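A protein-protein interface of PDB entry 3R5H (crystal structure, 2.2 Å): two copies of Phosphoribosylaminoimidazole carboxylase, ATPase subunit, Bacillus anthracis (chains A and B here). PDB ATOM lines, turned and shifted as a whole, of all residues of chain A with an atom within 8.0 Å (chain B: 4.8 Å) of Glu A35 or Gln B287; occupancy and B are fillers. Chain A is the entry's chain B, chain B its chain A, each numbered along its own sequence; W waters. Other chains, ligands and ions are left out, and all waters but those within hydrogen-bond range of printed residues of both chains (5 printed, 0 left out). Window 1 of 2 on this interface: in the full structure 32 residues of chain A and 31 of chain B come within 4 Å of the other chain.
The side-chain amide nitrogen (NE2) of Gln B287 is in hydrogen-bond range of the side-chain carboxylate (OE2) of Glu A35, 3.1 Å away. OE1 of Glu A35 lies within hydrogen-bond range of ND1 of His B342 (2.9 Å). The backbone NH (N) of Leu B343 lies within hydrogen-bond range of the backbone carbonyl oxygen (O) of Glu A35, 2.9 Å away.
The side-chain sulfur (SD) of Met B28 is in hydrogen-bond range of the side-chain amide nitrogen (NE2) of Gln B287 (3.5 Å). OE1 of Gln B287 is in hydrogen-bond range of ND1 of His B342 (3.3 Å). OE1 of Gln B287 lies within hydrogen-bond range of NE2 of His B357 (2.7 Å). A ring nitrogen (NE2) of His B342 sits at hydrogen-bond distance from the side-chain carboxylate (OD2) of Asp B288 (2.7 Å). The backbone carbonyl oxygen (O) of His B357 is in hydrogen-bond range of the backbone NH (N) of His B342 (2.8 Å).
Leu B341 touches Pro A13 (CD2 to CG, 3.9 Å). CB of Pro A13 touches CD1 of Leu B343, at 3.5 Å. Leu A31 touches Leu B31 (CD2 to CD2, 3.8 Å). Lys A34 touches Leu B343. Glu A35 touches Leu B31 (CD to CD1, 3.7 Å). Glu A35 touches Leu B341 (O to O, 3.9 Å). O of Leu B341 touches CG of Met A36, at 3.8 Å. Leu B343 touches Met A36 (CB to O, 3.6 Å). N of Gly A37 touches O of Leu B343 (3.5 Å).
Met A29 touches none of the printed residues of chain B. Of the printed residues of chain B, Leu A31 touches Leu B31 (3.8 Å). Printed residues of chain B within 4 Å of Lys A34: Leu B343 (3.9 Å). Glu A35 touches just these residues of chain B: Leu B31 (3.7 Å), Gln B287 (3.1 Å), Leu B341 (3.9 Å), His B342 (2.9 Å) and Leu B343 (2.9 Å). Of the printed residues of chain A, Leu B31 touches Leu A31 and Glu A35. Gln B287 touches just one residue of chain A: Glu A35. Ser B293 touches none of the printed residues of chain A. Printed residues of chain A within 4 Å of Leu B343: Pro A13 (3.5 Å), Lys A34 (3.9 Å), Glu A35 (2.9 Å), Met A36 (3.6 Å) and Gly A37 (3.5 Å). The nearest residue of chain A that does not touch Gln B287 is Glu A291 (6.7 Å). The nearest printed residue of chain A that does not touch His B342 is Met A36 (4.6 Å).
Of the 16 printed residues of chain B, 5 touch a printed residue of chain A. Printed residues of chain B that touch a printed residue of chain A: Leu B31, Gln B287, Leu B341, His B342 and Leu B343. Among the printed residues, no Asp or Glu carboxylate lies within 4 Å of a Lys or Arg side-chain nitrogen of the other chain.
Leu A31 touches its own counterpart, Leu B31.
Water W3 lies within hydrogen-bond range of the backbone carbonyl oxygen of Glu A291 (2.6 Å) and the side-chain carboxylate of Asp B288 (3.2 Å). Water W5 lies within hydrogen-bond range of O of Met B28 and OE2 of Glu A35. Water W4 lies within hydrogen-bond range of O of Leu B341 (2.7 Å) and NH2 of Arg A300 (3.2 Å). Water W2 bridges O of Leu B343 (3.0 Å) and O of Glu A35 (3.4 Å). Water W1 bridges N of Leu B341 and NH2 of Arg A300.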
ATOM      1  N   PRO A  13      11.071  12.073  -9.557  1.00  0.00           N
ATOM      2  CA  PRO A  13      10.428  12.673 -10.719  1.00  0.00           C
ATOM      3  C   PRO A  13       9.194  13.477 -10.318  1.00  0.00           C
ATOM      4  O   PRO A  13       8.389  13.005  -9.532  1.00  0.00           O
ATOM      5  CB  PRO A  13      10.026  11.452 -11.530  1.00  0.00           C
ATOM      6  CG  PRO A  13      11.188  10.537 -11.322  1.00  0.00           C
ATOM      7  CD  PRO A  13      11.488  10.686  -9.841  1.00  0.00           C
ATOM      8  N   MET A  29      21.368  19.356 -19.339  1.00  0.00           N
ATOM      9  CA  MET A  29      20.869  18.811 -18.072  1.00  0.00           C
ATOM     10  C   MET A  29      19.359  18.883 -18.004  1.00  0.00           C
ATOM     11  O   MET A  29      18.708  17.930 -17.578  1.00  0.00           O
ATOM     12  CB  MET A  29      21.406  19.616 -16.887  1.00  0.00           C
ATOM     13  CG  MET A  29      22.855  19.351 -16.518  1.00  0.00           C
ATOM     14  SD  MET A  29      23.231  20.338 -15.061  1.00  0.00           S
ATOM     15  CE  MET A  29      25.011  20.154 -14.988  1.00  0.00           C
ATOM     16  N   ALA A  30      18.816  20.044 -18.376  1.00  0.00           N
ATOM     17  CA  ALA A  30      17.383  20.312 -18.274  1.00  0.00           C
ATOM     18  C   ALA A  30      16.587  19.407 -19.222  1.00  0.00           C
ATOM     19  O   ALA A  30      15.592  18.814 -18.830  1.00  0.00           O
ATOM     20  CB  ALA A  30      17.099  21.794 -18.564  1.00  0.00           C
ATOM     21  N   LEU A  31      17.046  19.286 -20.462  1.00  0.00           N
ATOM     22  CA  LEU A  31      16.373  18.421 -21.435  1.00  0.00           C
ATOM     23  C   LEU A  31      16.353  16.969 -20.954  1.00  0.00           C
ATOM     24  O   LEU A  31      15.342  16.266 -21.092  1.00  0.00           O
ATOM     25  CB  LEU A  31      17.044  18.533 -22.813  1.00  0.00           C
ATOM     26  CG  LEU A  31      16.781  19.849 -23.555  1.00  0.00           C
ATOM     27  CD1 LEU A  31      17.745  20.018 -24.730  1.00  0.00           C
ATOM     28  CD2 LEU A  31      15.326  19.938 -24.034  1.00  0.00           C
ATOM     29  N   ALA A  32      17.460  16.535 -20.360  1.00  0.00           N
ATOM     30  CA  ALA A  32      17.547  15.183 -19.810  1.00  0.00           C
ATOM     31  C   ALA A  32      16.575  15.055 -18.637  1.00  0.00           C
ATOM     32  O   ALA A  32      15.805  14.093 -18.572  1.00  0.00           O
ATOM     33  CB  ALA A  32      19.011  14.848 -19.367  1.00  0.00           C
ATOM     34  N   ALA A  33      16.602  16.029 -17.726  1.00  0.00           N
ATOM     35  CA  ALA A  33      15.705  16.008 -16.566  1.00  0.00           C
ATOM     36  C   ALA A  33      14.218  15.997 -16.948  1.00  0.00           C
ATOM     37  O   ALA A  33      13.420  15.282 -16.337  1.00  0.00           O
ATOM     38  CB  ALA A  33      16.000  17.165 -15.643  1.00  0.00           C
ATOM     39  N   LYS A  34      13.842  16.773 -17.962  1.00  0.00           N
ATOM     40  CA  LYS A  34      12.429  16.835 -18.365  1.00  0.00           C
ATOM     41  C   LYS A  34      11.875  15.534 -18.933  1.00  0.00           C
ATOM     42  O   LYS A  34      10.673  15.301 -18.834  1.00  0.00           O
ATOM     43  CB  LYS A  34      12.166  17.982 -19.341  1.00  0.00           C
ATOM     44  CG  LYS A  34      12.206  19.343 -18.683  1.00  0.00           C
ATOM     45  CD  LYS A  34      11.150  20.212 -19.275  1.00  0.00           C
ATOM     46  CE  LYS A  34      10.930  21.435 -18.417  1.00  0.00           C
ATOM     47  NZ  LYS A  34       9.466  21.676 -18.210  1.00  0.00           N
ATOM     48  N   GLU A  35      12.723  14.691 -19.532  1.00  0.00           N
ATOM     49  CA  GLU A  35      12.231  13.416 -20.053  1.00  0.00           C
ATOM     50  C   GLU A  35      11.739  12.538 -18.914  1.00  0.00           C
ATOM     51  O   GLU A  35      10.798  11.762 -19.085  1.00  0.00           O
ATOM     52  CB  GLU A  35      13.254  12.689 -20.936  1.00  0.00           C
ATOM     53  CG  GLU A  35      13.270  13.215 -22.395  1.00  0.00           C
ATOM     54  CD  GLU A  35      12.254  12.567 -23.390  1.00  0.00           C
ATOM     55  OE1 GLU A  35      11.202  11.940 -23.000  1.00  0.00           O
ATOM     56  OE2 GLU A  35      12.546  12.740 -24.620  1.00  0.00           O
ATOM     57  N   MET A  36      12.351  12.699 -17.744  1.00  0.00           N
ATOM     58  CA  MET A  36      11.918  11.972 -16.546  1.00  0.00           C
ATOM     59  C   MET A  36      10.808  12.673 -15.761  1.00  0.00           C
ATOM     60  O   MET A  36      10.390  12.173 -14.736  1.00  0.00           O
ATOM     61  CB  MET A  36      13.106  11.687 -15.619  1.00  0.00           C
ATOM     62  CG  MET A  36      14.340  11.123 -16.328  1.00  0.00           C
ATOM     63  SD  MET A  36      15.586  10.521 -15.149  1.00  0.00           S
ATOM     64  CE  MET A  36      14.606   9.273 -14.338  1.00  0.00           C
ATOM     65  N   GLY A  37      10.344  13.827 -16.226  1.00  0.00           N
ATOM     66  CA  GLY A  37       9.242  14.517 -15.579  1.00  0.00           C
ATOM     67  C   GLY A  37       9.626  15.527 -14.499  1.00  0.00           C
ATOM     68  O   GLY A  37       8.753  16.013 -13.769  1.00  0.00           O
ATOM     69  N   TYR A  38      10.914  15.864 -14.396  1.00  0.00           N
ATOM     70  CA  TYR A  38      11.339  16.912 -13.472  1.00  0.00           C
ATOM     71  C   TYR A  38      10.973  18.287 -13.998  1.00  0.00           C
ATOM     72  O   TYR A  38      10.842  18.487 -15.204  1.00  0.00           O
ATOM     73  CB  TYR A  38      12.847  16.861 -13.217  1.00  0.00           C
ATOM     74  CG  TYR A  38      13.263  15.673 -12.420  1.00  0.00           C
ATOM     75  CD1 TYR A  38      13.189  15.686 -11.016  1.00  0.00           C
ATOM     76  CD2 TYR A  38      13.707  14.509 -13.053  1.00  0.00           C
ATOM     77  CE1 TYR A  38      13.566  14.565 -10.258  1.00  0.00           C
ATOM     78  CE2 TYR A  38      14.091  13.379 -12.301  1.00  0.00           C
ATOM     79  CZ  TYR A  38      14.017  13.423 -10.911  1.00  0.00           C
ATOM     80  OH  TYR A  38      14.381  12.318 -10.189  1.00  0.00           O
ATOM     81  N   ILE A  40      12.361  22.383 -13.896  1.00  0.00           N
ATOM     82  CA  ILE A  40      13.673  23.009 -13.940  1.00  0.00           C
ATOM     83  C   ILE A  40      13.573  24.482 -13.616  1.00  0.00           C
ATOM     84  O   ILE A  40      12.797  25.206 -14.257  1.00  0.00           O
ATOM     85  CB  ILE A  40      14.335  22.865 -15.351  1.00  0.00           C
ATOM     86  CG1 ILE A  40      14.564  21.398 -15.718  1.00  0.00           C
ATOM     87  CG2 ILE A  40      15.631  23.715 -15.453  1.00  0.00           C
ATOM     88  CD1 ILE A  40      15.409  20.618 -14.724  1.00  0.00           C
ATOM     89  N   GLN A 287      25.552  11.618 -25.683  1.00  0.00           N
ATOM     90  CA  GLN A 287      24.124  11.869 -25.967  1.00  0.00           C
ATOM     91  C   GLN A 287      23.614  10.916 -27.032  1.00  0.00           C
ATOM     92  O   GLN A 287      22.475  10.497 -26.988  1.00  0.00           O
ATOM     93  CB  GLN A 287      23.879  13.302 -26.434  1.00  0.00           C
ATOM     94  CG  GLN A 287      24.130  14.363 -25.395  1.00  0.00           C
ATOM     95  CD  GLN A 287      23.868  15.738 -25.953  1.00  0.00           C
ATOM     96  OE1 GLN A 287      24.626  16.222 -26.797  1.00  0.00           O
ATOM     97  NE2 GLN A 287      22.770  16.374 -25.510  1.00  0.00           N
ATOM     98  N   CYS A 290      25.998   6.491 -26.227  1.00  0.00           N
ATOM     99  CA  CYS A 290      25.922   5.672 -25.028  1.00  0.00           C
ATOM    100  C   CYS A 290      24.499   5.390 -24.643  1.00  0.00           C
ATOM    101  O   CYS A 290      23.585   6.083 -25.072  1.00  0.00           O
ATOM    102  CB  CYS A 290      26.661   6.330 -23.855  1.00  0.00           C
ATOM    103  SG  CYS A 290      28.438   6.336 -24.079  1.00  0.00           S
ATOM    104  N   GLU A 291      24.333   4.360 -23.824  1.00  0.00           N
ATOM    105  CA  GLU A 291      23.037   3.985 -23.286  1.00  0.00           C
ATOM    106  C   GLU A 291      22.435   5.140 -22.489  1.00  0.00           C
ATOM    107  O   GLU A 291      21.231   5.374 -22.557  1.00  0.00           O
ATOM    108  CB  GLU A 291      23.211   2.754 -22.407  1.00  0.00           C
ATOM    109  CG  GLU A 291      21.988   1.899 -22.321  1.00  0.00           C
ATOM    110  CD  GLU A 291      22.274   0.481 -21.853  1.00  0.00           C
ATOM    111  OE1 GLU A 291      21.473  -0.020 -21.020  1.00  0.00           O
ATOM    112  OE2 GLU A 291      23.287  -0.132 -22.310  1.00  0.00           O
ATOM    113  N   ARG A 300      20.559  11.738 -12.547  1.00  0.00           N
ATOM    114  CA  ARG A 300      20.353  10.535 -11.742  1.00  0.00           C
ATOM    115  C   ARG A 300      21.237  10.566 -10.491  1.00  0.00           C
ATOM    116  O   ARG A 300      20.782  10.200  -9.402  1.00  0.00           O
ATOM    117  CB  ARG A 300      20.610   9.265 -12.556  1.00  0.00           C
ATOM    118  CG  ARG A 300      19.505   8.919 -13.562  1.00  0.00           C
ATOM    119  CD  ARG A 300      19.966   7.885 -14.597  1.00  0.00           C
ATOM    120  NE  ARG A 300      18.829   7.380 -15.384  1.00  0.00           N
ATOM    121  CZ  ARG A 300      18.344   7.960 -16.490  1.00  0.00           C
ATOM    122  NH1 ARG A 300      18.888   9.072 -16.979  1.00  0.00           N
ATOM    123  NH2 ARG A 300      17.303   7.429 -17.122  1.00  0.00           N
ATOM    124  N   MET B  28       7.352  14.987 -26.676  1.00  0.00           N
ATOM    125  CA  MET B  28       8.556  14.284 -27.104  1.00  0.00           C
ATOM    126  C   MET B  28       9.102  14.765 -28.456  1.00  0.00           C
ATOM    127  O   MET B  28      10.327  14.817 -28.631  1.00  0.00           O
ATOM    128  CB  MET B  28       8.308  12.780 -27.048  1.00  0.00           C
ATOM    129  CG  MET B  28       8.127  12.316 -25.595  1.00  0.00           C
ATOM    130  SD  MET B  28       7.875  10.542 -25.344  1.00  0.00           S
ATOM    131  CE  MET B  28       6.180  10.391 -25.856  1.00  0.00           C
ATOM    132  N   LEU B  31      10.911  18.015 -27.459  1.00  0.00           N
ATOM    133  CA  LEU B  31      12.188  17.797 -26.789  1.00  0.00           C
ATOM    134  C   LEU B  31      13.255  17.389 -27.806  1.00  0.00           C
ATOM    135  O   LEU B  31      14.416  17.808 -27.696  1.00  0.00           O
ATOM    136  CB  LEU B  31      12.072  16.751 -25.660  1.00  0.00           C
ATOM    137  CG  LEU B  31      11.259  17.194 -24.430  1.00  0.00           C
ATOM    138  CD1 LEU B  31      10.809  15.999 -23.599  1.00  0.00           C
ATOM    139  CD2 LEU B  31      12.025  18.213 -23.560  1.00  0.00           C
ATOM    140  N   GLY B 283       6.199   2.922 -30.693  1.00  0.00           N
ATOM    141  CA  GLY B 283       7.487   3.365 -31.147  1.00  0.00           C
ATOM    142  C   GLY B 283       8.316   4.045 -30.094  1.00  0.00           C
ATOM    143  O   GLY B 283       9.409   4.523 -30.398  1.00  0.00           O
ATOM    144  N   HIS B 284       7.815   4.117 -28.859  1.00  0.00           N
ATOM    145  CA  HIS B 284       8.540   4.825 -27.800  1.00  0.00           C
ATOM    146  C   HIS B 284       9.837   4.133 -27.415  1.00  0.00           C
ATOM    147  O   HIS B 284      10.709   4.759 -26.813  1.00  0.00           O
ATOM    148  CB  HIS B 284       7.702   4.970 -26.517  1.00  0.00           C
ATOM    149  CG  HIS B 284       6.526   5.883 -26.650  1.00  0.00           C
ATOM    150  ND1 HIS B 284       6.350   6.719 -27.730  1.00  0.00           N
ATOM    151  CD2 HIS B 284       5.482   6.115 -25.819  1.00  0.00           C
ATOM    152  CE1 HIS B 284       5.236   7.415 -27.566  1.00  0.00           C
ATOM    153  NE2 HIS B 284       4.690   7.059 -26.417  1.00  0.00           N
ATOM    154  N   TYR B 285       9.943   2.840 -27.722  1.00  0.00           N
ATOM    155  CA  TYR B 285      11.172   2.108 -27.438  1.00  0.00           C
ATOM    156  C   TYR B 285      12.366   2.783 -28.112  1.00  0.00           C
ATOM    157  O   TYR B 285      13.497   2.670 -27.653  1.00  0.00           O
ATOM    158  CB  TYR B 285      11.057   0.654 -27.907  1.00  0.00           C
ATOM    159  CG  TYR B 285      11.143   0.477 -29.404  1.00  0.00           C
ATOM    160  CD1 TYR B 285       9.995   0.461 -30.195  1.00  0.00           C
ATOM    161  CD2 TYR B 285      12.376   0.308 -30.029  1.00  0.00           C
ATOM    162  CE1 TYR B 285      10.085   0.298 -31.599  1.00  0.00           C
ATOM    163  CE2 TYR B 285      12.482   0.139 -31.413  1.00  0.00           C
ATOM    164  CZ  TYR B 285      11.335   0.131 -32.189  1.00  0.00           C
ATOM    165  OH  TYR B 285      11.459  -0.036 -33.554  1.00  0.00           O
ATOM    166  N   THR B 286      12.107   3.470 -29.221  1.00  0.00           N
ATOM    167  CA  THR B 286      13.160   4.014 -30.064  1.00  0.00           C
ATOM    168  C   THR B 286      13.971   5.112 -29.359  1.00  0.00           C
ATOM    169  O   THR B 286      15.108   5.377 -29.740  1.00  0.00           O
ATOM    170  CB  THR B 286      12.580   4.604 -31.371  1.00  0.00           C
ATOM    171  OG1 THR B 286      11.624   5.635 -31.049  1.00  0.00           O
ATOM    172  CG2 THR B 286      11.908   3.516 -32.240  1.00  0.00           C
ATOM    173  N   GLN B 287      13.392   5.740 -28.339  1.00  0.00           N
ATOM    174  CA  GLN B 287      14.075   6.798 -27.575  1.00  0.00           C
ATOM    175  C   GLN B 287      15.382   6.337 -26.953  1.00  0.00           C
ATOM    176  O   GLN B 287      16.347   7.102 -26.871  1.00  0.00           O
ATOM    177  CB  GLN B 287      13.169   7.314 -26.465  1.00  0.00           C
ATOM    178  CG  GLN B 287      12.011   8.181 -26.973  1.00  0.00           C
ATOM    179  CD  GLN B 287      11.253   8.773 -25.826  1.00  0.00           C
ATOM    180  OE1 GLN B 287      10.608   8.055 -25.059  1.00  0.00           O
ATOM    181  NE2 GLN B 287      11.349  10.077 -25.670  1.00  0.00           N
ATOM    182  N   ASP B 288      15.418   5.082 -26.524  1.00  0.00           N
ATOM    183  CA  ASP B 288      16.573   4.587 -25.803  1.00  0.00           C
ATOM    184  C   ASP B 288      17.316   3.474 -26.532  1.00  0.00           C
ATOM    185  O   ASP B 288      18.490   3.259 -26.255  1.00  0.00           O
ATOM    186  CB  ASP B 288      16.153   4.140 -24.408  1.00  0.00           C
ATOM    187  CG  ASP B 288      15.680   5.305 -23.544  1.00  0.00           C
ATOM    188  OD1 ASP B 288      16.504   6.201 -23.242  1.00  0.00           O
ATOM    189  OD2 ASP B 288      14.486   5.319 -23.164  1.00  0.00           O
ATOM    190  N   ALA B 289      16.651   2.789 -27.469  1.00  0.00           N
ATOM    191  CA  ALA B 289      17.230   1.588 -28.086  1.00  0.00           C
ATOM    192  C   ALA B 289      17.739   1.757 -29.516  1.00  0.00           C
ATOM    193  O   ALA B 289      18.479   0.903 -30.013  1.00  0.00           O
ATOM    194  CB  ALA B 289      16.249   0.414 -28.016  1.00  0.00           C
ATOM    195  N   SER B 293      15.386   8.479 -32.459  1.00  0.00           N
ATOM    196  CA  SER B 293      14.036   8.195 -31.981  1.00  0.00           C
ATOM    197  C   SER B 293      12.996   8.481 -33.072  1.00  0.00           C
ATOM    198  O   SER B 293      13.277   9.187 -34.030  1.00  0.00           O
ATOM    199  CB  SER B 293      13.707   8.997 -30.716  1.00  0.00           C
ATOM    200  OG  SER B 293      13.369  10.328 -31.036  1.00  0.00           O
ATOM    201  N   PHE B 295      10.757  10.451 -32.750  1.00  0.00           N
ATOM    202  CA  PHE B 295      10.466  11.868 -32.672  1.00  0.00           C
ATOM    203  C   PHE B 295      11.506  12.716 -33.369  1.00  0.00           C
ATOM    204  O   PHE B 295      11.164  13.662 -34.063  1.00  0.00           O
ATOM    205  CB  PHE B 295      10.287  12.301 -31.208  1.00  0.00           C
ATOM    206  CG  PHE B 295       9.268  11.484 -30.456  1.00  0.00           C
ATOM    207  CD1 PHE B 295       9.675  10.471 -29.580  1.00  0.00           C
ATOM    208  CD2 PHE B 295       7.907  11.727 -30.621  1.00  0.00           C
ATOM    209  CE1 PHE B 295       8.749   9.706 -28.894  1.00  0.00           C
ATOM    210  CE2 PHE B 295       6.944  10.958 -29.937  1.00  0.00           C
ATOM    211  CZ  PHE B 295       7.364   9.941 -29.080  1.00  0.00           C
ATOM    212  N   LEU B 341      13.376   5.702 -17.646  1.00  0.00           N
ATOM    213  CA  LEU B 341      12.073   6.226 -17.291  1.00  0.00           C
ATOM    214  C   LEU B 341      11.717   7.495 -18.060  1.00  0.00           C
ATOM    215  O   LEU B 341      12.538   8.413 -18.199  1.00  0.00           O
ATOM    216  CB  LEU B 341      12.041   6.478 -15.780  1.00  0.00           C
ATOM    217  CG  LEU B 341      10.753   7.035 -15.162  1.00  0.00           C
ATOM    218  CD1 LEU B 341       9.636   6.014 -15.328  1.00  0.00           C
ATOM    219  CD2 LEU B 341      10.940   7.397 -13.686  1.00  0.00           C
ATOM    220  N   HIS B 342      10.489   7.533 -18.571  1.00  0.00           N
ATOM    221  CA  HIS B 342       9.949   8.724 -19.222  1.00  0.00           C
ATOM    222  C   HIS B 342       8.608   9.063 -18.589  1.00  0.00           C
ATOM    223  O   HIS B 342       7.717   8.224 -18.552  1.00  0.00           O
ATOM    224  CB  HIS B 342       9.802   8.506 -20.740  1.00  0.00           C
ATOM    225  CG  HIS B 342      11.102   8.227 -21.433  1.00  0.00           C
ATOM    226  ND1 HIS B 342      11.785   9.187 -22.153  1.00  0.00           N
ATOM    227  CD2 HIS B 342      11.867   7.108 -21.478  1.00  0.00           C
ATOM    228  CE1 HIS B 342      12.906   8.668 -22.623  1.00  0.00           C
ATOM    229  NE2 HIS B 342      12.983   7.408 -22.227  1.00  0.00           N
ATOM    230  N   LEU B 343       8.481  10.271 -18.048  1.00  0.00           N
ATOM    231  CA  LEU B 343       7.206  10.719 -17.463  1.00  0.00           C
ATOM    232  C   LEU B 343       6.817  12.029 -18.110  1.00  0.00           C
ATOM    233  O   LEU B 343       7.666  12.876 -18.325  1.00  0.00           O
ATOM    234  CB  LEU B 343       7.291  10.839 -15.936  1.00  0.00           C
ATOM    235  CG  LEU B 343       7.475   9.492 -15.197  1.00  0.00           C
ATOM    236  CD1 LEU B 343       7.868   9.720 -13.733  1.00  0.00           C
ATOM    237  CD2 LEU B 343       6.231   8.578 -15.293  1.00  0.00           C
ATOM    238  N   HIS B 357       6.282   6.039 -19.661  1.00  0.00           N
ATOM    239  CA  HIS B 357       6.688   4.713 -20.085  1.00  0.00           C
ATOM    240  C   HIS B 357       8.109   4.441 -19.609  1.00  0.00           C
ATOM    241  O   HIS B 357       8.895   5.370 -19.388  1.00  0.00           O
ATOM    242  CB  HIS B 357       6.577   4.537 -21.620  1.00  0.00           C
ATOM    243  CG  HIS B 357       7.539   5.377 -22.417  1.00  0.00           C
ATOM    244  ND1 HIS B 357       7.200   6.614 -22.930  1.00  0.00           N
ATOM    245  CD2 HIS B 357       8.813   5.139 -22.818  1.00  0.00           C
ATOM    246  CE1 HIS B 357       8.234   7.113 -23.586  1.00  0.00           C
ATOM    247  NE2 HIS B 357       9.224   6.234 -23.538  1.00  0.00           N
ATOM    248  N   ASN B 359      11.570   2.195 -20.597  1.00  0.00           N
ATOM    249  CA  ASN B 359      12.262   1.372 -21.564  1.00  0.00           C
ATOM    250  C   ASN B 359      13.283   0.523 -20.817  1.00  0.00           C
ATOM    251  O   ASN B 359      14.192   1.057 -20.214  1.00  0.00           O
ATOM    252  CB  ASN B 359      12.955   2.261 -22.605  1.00  0.00           C
ATOM    253  CG  ASN B 359      11.989   2.809 -23.649  1.00  0.00           C
ATOM    254  OD1 ASN B 359      11.004   2.168 -23.970  1.00  0.00           O
ATOM    255  ND2 ASN B 359      12.282   3.987 -24.192  1.00  0.00           N
HETATM  256  O   HOH W   1      15.316   5.888 -15.170  1.00  0.00           O
HETATM  257  O   HOH W   2       8.641  13.391 -21.120  1.00  0.00           O
HETATM  258  O   HOH W   3      19.271   6.904 -21.861  1.00  0.00           O
HETATM  259  O   HOH W   4      15.106   8.804 -19.042  1.00  0.00           O
HETATM  260  O   HOH W   5      12.010  13.008 -27.472  1.00  0.00           O
